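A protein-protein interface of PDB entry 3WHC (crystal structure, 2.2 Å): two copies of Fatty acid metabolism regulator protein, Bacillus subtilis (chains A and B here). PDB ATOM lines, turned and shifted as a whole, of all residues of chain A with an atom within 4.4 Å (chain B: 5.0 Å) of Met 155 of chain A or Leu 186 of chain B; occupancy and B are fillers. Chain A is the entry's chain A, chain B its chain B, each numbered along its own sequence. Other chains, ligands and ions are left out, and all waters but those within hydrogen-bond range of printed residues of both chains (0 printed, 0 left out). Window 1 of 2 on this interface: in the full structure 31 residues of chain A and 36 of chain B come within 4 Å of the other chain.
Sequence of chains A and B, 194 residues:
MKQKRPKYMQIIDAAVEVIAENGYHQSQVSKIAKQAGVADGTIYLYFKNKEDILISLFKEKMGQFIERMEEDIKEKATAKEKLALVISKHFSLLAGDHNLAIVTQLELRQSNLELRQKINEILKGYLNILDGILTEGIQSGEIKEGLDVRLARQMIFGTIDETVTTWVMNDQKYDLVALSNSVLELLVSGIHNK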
ATOM      1  N   LEU A 147       3.763  -6.541 -14.486  1.00  0.00           N
ATOM      2  CA  LEU A 147       3.382  -7.410 -13.377  1.00  0.00           C
ATOM      3  C   LEU A 147       1.869  -7.382 -13.186  1.00  0.00           C
ATOM      4  O   LEU A 147       1.276  -6.311 -13.036  1.00  0.00           O
ATOM      5  CB  LEU A 147       4.082  -6.989 -12.082  1.00  0.00           C
ATOM      6  CG  LEU A 147       3.909  -7.905 -10.864  1.00  0.00           C
ATOM      7  CD1 LEU A 147       5.031  -8.930 -10.792  1.00  0.00           C
ATOM      8  CD2 LEU A 147       3.860  -7.090  -9.583  1.00  0.00           C
ATOM      9  N   LEU A 151      -2.702 -11.058  -9.401  1.00  0.00           N
ATOM     10  CA  LEU A 151      -2.021 -12.334  -9.181  1.00  0.00           C
ATOM     11  C   LEU A 151      -0.863 -12.234  -8.189  1.00  0.00           C
ATOM     12  O   LEU A 151      -0.641 -13.155  -7.400  1.00  0.00           O
ATOM     13  CB  LEU A 151      -1.539 -12.930 -10.508  1.00  0.00           C
ATOM     14  CG  LEU A 151      -2.564 -13.731 -11.318  1.00  0.00           C
ATOM     15  CD1 LEU A 151      -2.029 -14.019 -12.710  1.00  0.00           C
ATOM     16  CD2 LEU A 151      -2.942 -15.027 -10.611  1.00  0.00           C
ATOM     17  N   ALA A 152      -0.136 -11.119  -8.237  1.00  0.00           N
ATOM     18  CA  ALA A 152       0.957 -10.857  -7.299  1.00  0.00           C
ATOM     19  C   ALA A 152       0.434 -10.711  -5.868  1.00  0.00           C
ATOM     20  O   ALA A 152       1.024 -11.250  -4.931  1.00  0.00           O
ATOM     21  CB  ALA A 152       1.732  -9.616  -7.721  1.00  0.00           C
ATOM     22  N   ARG A 153      -0.675  -9.987  -5.724  1.00  0.00           N
ATOM     23  CA  ARG A 153      -1.403  -9.846  -4.459  1.00  0.00           C
ATOM     24  C   ARG A 153      -1.862 -11.207  -3.924  1.00  0.00           C
ATOM     25  O   ARG A 153      -1.695 -11.506  -2.738  1.00  0.00           O
ATOM     26  CB  ARG A 153      -2.610  -8.929  -4.673  1.00  0.00           C
ATOM     27  CG  ARG A 153      -3.604  -8.860  -3.524  1.00  0.00           C
ATOM     28  CD  ARG A 153      -5.035  -8.819  -4.043  1.00  0.00           C
ATOM     29  NE  ARG A 153      -5.228  -7.784  -5.059  1.00  0.00           N
ATOM     30  CZ  ARG A 153      -6.337  -7.622  -5.774  1.00  0.00           C
ATOM     31  NH1 ARG A 153      -7.380  -8.426  -5.595  1.00  0.00           N
ATOM     32  NH2 ARG A 153      -6.406  -6.650  -6.674  1.00  0.00           N
ATOM     33  N   GLN A 154      -2.442 -12.018  -4.811  1.00  0.00           N
ATOM     34  CA  GLN A 154      -2.900 -13.365  -4.473  1.00  0.00           C
ATOM     35  C   GLN A 154      -1.737 -14.267  -4.063  1.00  0.00           C
ATOM     36  O   GLN A 154      -1.882 -15.099  -3.165  1.00  0.00           O
ATOM     37  CB  GLN A 154      -3.676 -13.981  -5.643  1.00  0.00           C
ATOM     38  CG  GLN A 154      -5.079 -13.414  -5.819  1.00  0.00           C
ATOM     39  CD  GLN A 154      -5.644 -13.636  -7.212  1.00  0.00           C
ATOM     40  OE1 GLN A 154      -5.569 -14.735  -7.764  1.00  0.00           O
ATOM     41  NE2 GLN A 154      -6.220 -12.587  -7.785  1.00  0.00           N
ATOM     42  N   MET A 155      -0.589 -14.088  -4.721  1.00  0.00           N
ATOM     43  CA  MET A 155       0.637 -14.798  -4.365  1.00  0.00           C
ATOM     44  C   MET A 155       1.121 -14.418  -2.966  1.00  0.00           C
ATOM     45  O   MET A 155       1.401 -15.294  -2.149  1.00  0.00           O
ATOM     46  CB  MET A 155       1.743 -14.532  -5.390  1.00  0.00           C
ATOM     47  CG  MET A 155       3.090 -15.124  -5.006  1.00  0.00           C
ATOM     48  SD  MET A 155       4.364 -14.825  -6.239  1.00  0.00           S
ATOM     49  CE  MET A 155       5.783 -15.606  -5.480  1.00  0.00           C
ATOM     50  N   ILE A 156       1.216 -13.115  -2.703  1.00  0.00           N
ATOM     51  CA  ILE A 156       1.696 -12.608  -1.415  1.00  0.00           C
ATOM     52  C   ILE A 156       0.811 -13.087  -0.259  1.00  0.00           C
ATOM     53  O   ILE A 156       1.296 -13.744   0.663  1.00  0.00           O
ATOM     54  CB  ILE A 156       1.829 -11.066  -1.410  1.00  0.00           C
ATOM     55  CG1 ILE A 156       2.924 -10.618  -2.389  1.00  0.00           C
ATOM     56  CG2 ILE A 156       2.144 -10.556  -0.009  1.00  0.00           C
ATOM     57  CD1 ILE A 156       2.839  -9.161  -2.798  1.00  0.00           C
ATOM     58  N   PHE A 157      -0.482 -12.772  -0.321  1.00  0.00           N
ATOM     59  CA  PHE A 157      -1.416 -13.172   0.729  1.00  0.00           C
ATOM     60  C   PHE A 157      -1.464 -14.688   0.904  1.00  0.00           C
ATOM     61  O   PHE A 157      -1.405 -15.181   2.027  1.00  0.00           O
ATOM     62  CB  PHE A 157      -2.821 -12.619   0.472  1.00  0.00           C
ATOM     63  CG  PHE A 157      -3.845 -13.078   1.478  1.00  0.00           C
ATOM     64  CD1 PHE A 157      -3.812 -12.610   2.788  1.00  0.00           C
ATOM     65  CD2 PHE A 157      -4.839 -13.979   1.116  1.00  0.00           C
ATOM     66  CE1 PHE A 157      -4.752 -13.030   3.716  1.00  0.00           C
ATOM     67  CE2 PHE A 157      -5.784 -14.402   2.040  1.00  0.00           C
ATOM     68  CZ  PHE A 157      -5.739 -13.928   3.342  1.00  0.00           C
ATOM     69  N   GLY A 158      -1.559 -15.411  -0.211  1.00  0.00           N
ATOM     70  CA  GLY A 158      -1.585 -16.876  -0.201  1.00  0.00           C
ATOM     71  C   GLY A 158      -0.379 -17.496   0.482  1.00  0.00           C
ATOM     72  O   GLY A 158      -0.518 -18.458   1.243  1.00  0.00           O
ATOM     73  N   THR A 159       0.801 -16.935   0.209  1.00  0.00           N
ATOM     74  CA  THR A 159       2.059 -17.392   0.808  1.00  0.00           C
ATOM     75  C   THR A 159       2.092 -17.125   2.313  1.00  0.00           C
ATOM     76  O   THR A 159       2.354 -18.036   3.102  1.00  0.00           O
ATOM     77  CB  THR A 159       3.280 -16.729   0.133  1.00  0.00           C
ATOM     78  OG1 THR A 159       3.280 -17.035  -1.266  1.00  0.00           O
ATOM     79  CG2 THR A 159       4.587 -17.209   0.757  1.00  0.00           C
ATOM     80  N   LEU A 187       9.143 -14.341  -1.889  1.00  0.00           N
ATOM     81  CA  LEU A 187       8.172 -13.541  -2.633  1.00  0.00           C
ATOM     82  C   LEU A 187       8.846 -12.533  -3.566  1.00  0.00           C
ATOM     83  O   LEU A 187       8.362 -12.280  -4.670  1.00  0.00           O
ATOM     84  CB  LEU A 187       7.225 -12.813  -1.674  1.00  0.00           C
ATOM     85  CG  LEU A 187       6.187 -13.644  -0.914  1.00  0.00           C
ATOM     86  CD1 LEU A 187       5.498 -12.788   0.138  1.00  0.00           C
ATOM     87  CD2 LEU A 187       5.168 -14.260  -1.865  1.00  0.00           C
ATOM     88  N   MET B 155       4.810 -21.547  -0.099  1.00  0.00           N
ATOM     89  CA  MET B 155       4.617 -20.461  -1.061  1.00  0.00           C
ATOM     90  C   MET B 155       3.934 -20.977  -2.327  1.00  0.00           C
ATOM     91  O   MET B 155       2.929 -20.418  -2.762  1.00  0.00           O
ATOM     92  CB  MET B 155       5.947 -19.780  -1.416  1.00  0.00           C
ATOM     93  CG  MET B 155       5.803 -18.680  -2.462  1.00  0.00           C
ATOM     94  SD  MET B 155       7.325 -17.816  -2.905  1.00  0.00           S
ATOM     95  CE  MET B 155       8.134 -19.044  -3.923  1.00  0.00           C
ATOM     96  N   THR B 159       0.119 -20.025  -3.048  1.00  0.00           N
ATOM     97  CA  THR B 159      -0.095 -19.185  -4.226  1.00  0.00           C
ATOM     98  C   THR B 159      -1.108 -19.803  -5.192  1.00  0.00           C
ATOM     99  O   THR B 159      -2.047 -19.127  -5.621  1.00  0.00           O
ATOM    100  CB  THR B 159       1.236 -18.906  -4.953  1.00  0.00           C
ATOM    101  OG1 THR B 159       2.116 -18.202  -4.070  1.00  0.00           O
ATOM    102  CG2 THR B 159       1.024 -18.080  -6.213  1.00  0.00           C
ATOM    103  N   SER B 182       1.428 -17.314 -15.893  1.00  0.00           N
ATOM    104  CA  SER B 182       1.641 -16.113 -15.088  1.00  0.00           C
ATOM    105  C   SER B 182       1.936 -16.464 -13.628  1.00  0.00           C
ATOM    106  O   SER B 182       2.787 -15.836 -12.997  1.00  0.00           O
ATOM    107  CB  SER B 182       0.433 -15.178 -15.178  1.00  0.00           C
ATOM    108  OG  SER B 182       0.232 -14.728 -16.504  1.00  0.00           O
ATOM    109  N   VAL B 183       1.235 -17.471 -13.106  1.00  0.00           N
ATOM    110  CA  VAL B 183       1.477 -17.984 -11.753  1.00  0.00           C
ATOM    111  C   VAL B 183       2.876 -18.605 -11.653  1.00  0.00           C
ATOM    112  O   VAL B 183       3.597 -18.364 -10.681  1.00  0.00           O
ATOM    113  CB  VAL B 183       0.381 -18.991 -11.310  1.00  0.00           C
ATOM    114  CG1 VAL B 183       0.784 -19.731 -10.040  1.00  0.00           C
ATOM    115  CG2 VAL B 183      -0.948 -18.278 -11.093  1.00  0.00           C
ATOM    116  N   LEU B 184       3.255 -19.384 -12.667  1.00  0.00           N
ATOM    117  CA  LEU B 184       4.571 -20.030 -12.719  1.00  0.00           C
ATOM    118  C   LEU B 184       5.724 -19.024 -12.675  1.00  0.00           C
ATOM    119  O   LEU B 184       6.659 -19.186 -11.885  1.00  0.00           O
ATOM    120  CB  LEU B 184       4.696 -20.916 -13.967  1.00  0.00           C
ATOM    121  CG  LEU B 184       6.065 -21.550 -14.259  1.00  0.00           C
ATOM    122  CD1 LEU B 184       6.340 -22.745 -13.352  1.00  0.00           C
ATOM    123  CD2 LEU B 184       6.177 -21.949 -15.723  1.00  0.00           C
ATOM    124  N   GLU B 185       5.649 -18.001 -13.527  1.00  0.00           N
ATOM    125  CA  GLU B 185       6.682 -16.965 -13.615  1.00  0.00           C
ATOM    126  C   GLU B 185       6.850 -16.203 -12.303  1.00  0.00           C
ATOM    127  O   GLU B 185       7.974 -15.904 -11.897  1.00  0.00           O
ATOM    128  CB  GLU B 185       6.387 -15.985 -14.760  1.00  0.00           C
ATOM    129  CG  GLU B 185       6.481 -16.584 -16.158  1.00  0.00           C
ATOM    130  CD  GLU B 185       7.890 -17.009 -16.543  1.00  0.00           C
ATOM    131  OE1 GLU B 185       8.867 -16.375 -16.084  1.00  0.00           O
ATOM    132  OE2 GLU B 185       8.022 -17.977 -17.323  1.00  0.00           O
ATOM    133  N   LEU B 186       5.728 -15.894 -11.653  1.00  0.00           N
ATOM    134  CA  LEU B 186       5.733 -15.229 -10.348  1.00  0.00           C
ATOM    135  C   LEU B 186       6.462 -16.052  -9.288  1.00  0.00           C
ATOM    136  O   LEU B 186       7.229 -15.512  -8.496  1.00  0.00           O
ATOM    137  CB  LEU B 186       4.302 -14.937  -9.882  1.00  0.00           C
ATOM    138  CG  LEU B 186       3.514 -13.811 -10.554  1.00  0.00           C
ATOM    139  CD1 LEU B 186       2.043 -13.926 -10.187  1.00  0.00           C
ATOM    140  CD2 LEU B 186       4.055 -12.438 -10.182  1.00  0.00           C
ATOM    141  N   LEU B 187       6.219 -17.359  -9.288  1.00  0.00           N
ATOM    142  CA  LEU B 187       6.850 -18.271  -8.336  1.00  0.00           C
ATOM    143  C   LEU B 187       8.326 -18.510  -8.648  1.00  0.00           C
ATOM    144  O   LEU B 187       9.126 -18.763  -7.744  1.00  0.00           O
ATOM    145  CB  LEU B 187       6.093 -19.602  -8.289  1.00  0.00           C
ATOM    146  CG  LEU B 187       4.684 -19.585  -7.682  1.00  0.00           C
ATOM    147  CD1 LEU B 187       3.976 -20.913  -7.915  1.00  0.00           C
ATOM    148  CD2 LEU B 187       4.724 -19.248  -6.197  1.00  0.00           C
ATOM    149  N   VAL B 188       8.678 -18.422  -9.929  1.00  0.00           N
ATOM    150  CA  VAL B 188      10.051 -18.635 -10.384  1.00  0.00           C
ATOM    151  C   VAL B 188      10.953 -17.429 -10.086  1.00  0.00           C
ATOM    152  O   VAL B 188      12.040 -17.589  -9.526  1.00  0.00           O
ATOM    153  CB  VAL B 188      10.091 -19.036 -11.884  1.00  0.00           C
ATOM    154  CG1 VAL B 188      11.470 -18.826 -12.495  1.00  0.00           C
ATOM    155  CG2 VAL B 188       9.655 -20.485 -12.057  1.00  0.00           C
ATOM    156  N   SER B 189      10.483 -16.230 -10.431  1.00  0.00           N
ATOM    157  CA  SER B 189      11.322 -15.024 -10.389  1.00  0.00           C
ATOM    158  C   SER B 189      10.942 -13.997  -9.318  1.00  0.00           C
ATOM    159  O   SER B 189      11.684 -13.039  -9.085  1.00  0.00           O
ATOM    160  CB  SER B 189      11.345 -14.351 -11.764  1.00  0.00           C
ATOM    161  OG  SER B 189      11.929 -15.202 -12.731  1.00  0.00           O
ATOM    162  N   GLY B 190       9.792 -14.193  -8.676  1.00  0.00           N
ATOM    163  CA  GLY B 190       9.329 -13.283  -7.629  1.00  0.00           C
ATOM    164  C   GLY B 190       8.747 -11.985  -8.161  1.00  0.00           C
ATOM    165  O   GLY B 190       8.643 -11.792  -9.375  1.00  0.00           O
ATOM    166  N   ILE B 191       8.369 -11.093  -7.249  1.00  0.00           N
ATOM    167  CA  ILE B 191       7.747  -9.817  -7.623  1.00  0.00           C
ATOM    168  C   ILE B 191       8.751  -8.789  -8.149  1.00  0.00           C
ATOM    169  O   ILE B 191       8.378  -7.868  -8.876  1.00  0.00           O
ATOM    170  CB  ILE B 191       6.881  -9.221  -6.481  1.00  0.00           C
ATOM    171  CG1 ILE B 191       7.683  -9.045  -5.186  1.00  0.00           C
ATOM    172  CG2 ILE B 191       5.654 -10.087  -6.233  1.00  0.00           C
ATOM    173  CD1 ILE B 191       8.228  -7.648  -4.972  1.00  0.00           C
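Met 155 of chain B touches its own counterpart, Met 155 of chain A.
Met 155 of chain A touches Thr 159 of chain B, and with the chains exchanged Thr 159 of chain A touches Met 155 of chain B.
Met 155 of chain A touches Leu 187 of chain B, but with the chains exchanged Leu 187 of chain A does not touch Met 155 of chain B (4.1 Å).
Thr 159 of chain A touches its own counterpart, Thr 159 of chain B.
Positions printed for both chains: 155, 159 and 187.
Of the 12 pairs that touch across the chains among the printed residues, 4 have their exchanged pair printed and touching as well.
The backbone carbonyl oxygen of Met 155 of chain A is in hydrogen-bond range of the side-chain hydroxyl of Thr 159 of chain A (2.7 Å).
The backbone carbonyl oxygen of Met 155 of chain B lies within hydrogen-bond range of the side-chain hydroxyl of Thr 159 of chain B (2.7 Å).
The side-chain hydroxyl (OG1) of Thr 159 of chain B lies within hydrogen-bond range of the side-chain hydroxyl (OG1) of Thr 159 of chain A, at 3.3 Å.
O of Leu 187 of chain A lies within hydrogen-bond range of N of Ile 191 of chain B.
SD of Met 155 of chain A sits close to O of Leu 186 of chain B, 3.7 Å away.
Of the 11 printed residues of chain A, 5 touch a printed residue of chain B.
Hydrophobic or aromatic side chains of chain A within 4 Å of the printed part of chain B: Leu 147, Leu 151 and Met 155.
Printed residues of chain B that touch a printed residue of chain A: Met 155, Thr 159, Ser 182, Val 183, Leu 186, Leu 187, Gly 190 and Ile 191.
Among the printed residues, 12 pairs touch across the chains.
Among the printed residues, no Asp or Glu carboxylate lies within 4 Å of a Lys or Arg side-chain nitrogen of the other chain.
Among the printed residues, merely in contact across the chains: Leu 147 of chain A with Leu 186 of chain B (3.7 Å), Leu 151 of chain A with Ser 182 of chain B (3.7 Å), Leu 151 of chain A with Val 183 of chain B (3.8 Å), Leu 151 of chain A with Leu 186 of chain B (3.7 Å), Met 155 of chain A with Met 155 of chain B (3.7 Å), Met 155 of chain A with Thr 159 of chain B (3.4 Å), Met 155 of chain A with Leu 187 of chain B (3.9 Å), Thr 159 of chain A with Met 155 of chain B (3.2 Å) and Leu 187 of chain A with Gly 190 of chain B (3.3 Å).
Met 155 of chain A touches just these residues of chain B: Met 155 (3.7 Å), Thr 159 (3.4 Å), Leu 186 (3.3 Å) and Leu 187 (3.9 Å).
Of chain A, only Leu 147 (3.7 Å), Leu 151 (3.7 Å) and Met 155 (3.3 Å) come within 4 Å of Leu 186 of chain B.
Of the printed residues of chain B, Leu 187 of chain A touches Gly 190 and Ile 191.
Printed residues of chain A within 4 Å of Ile 191 of chain B: Leu 187 (2.8 Å).
Of the printed residues of chain B, Leu 147 of chain A touches Leu 186 (3.7 Å).
Printed residues of chain B within 4 Å of Leu 151 of chain A: Ser 182, Val 183 and Leu 186.
Ser 189 of chain B touches none of the printed residues of chain A.
Arg 153 of chain A touches none of the printed residues of chain B.
The nearest residue of chain A that does not touch Leu 186 of chain B is Ala 152 of chain A (4.1 Å).
The nearest printed residue of chain A that does not touch Val 183 of chain B is Met 155 of chain A (5.7 Å).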
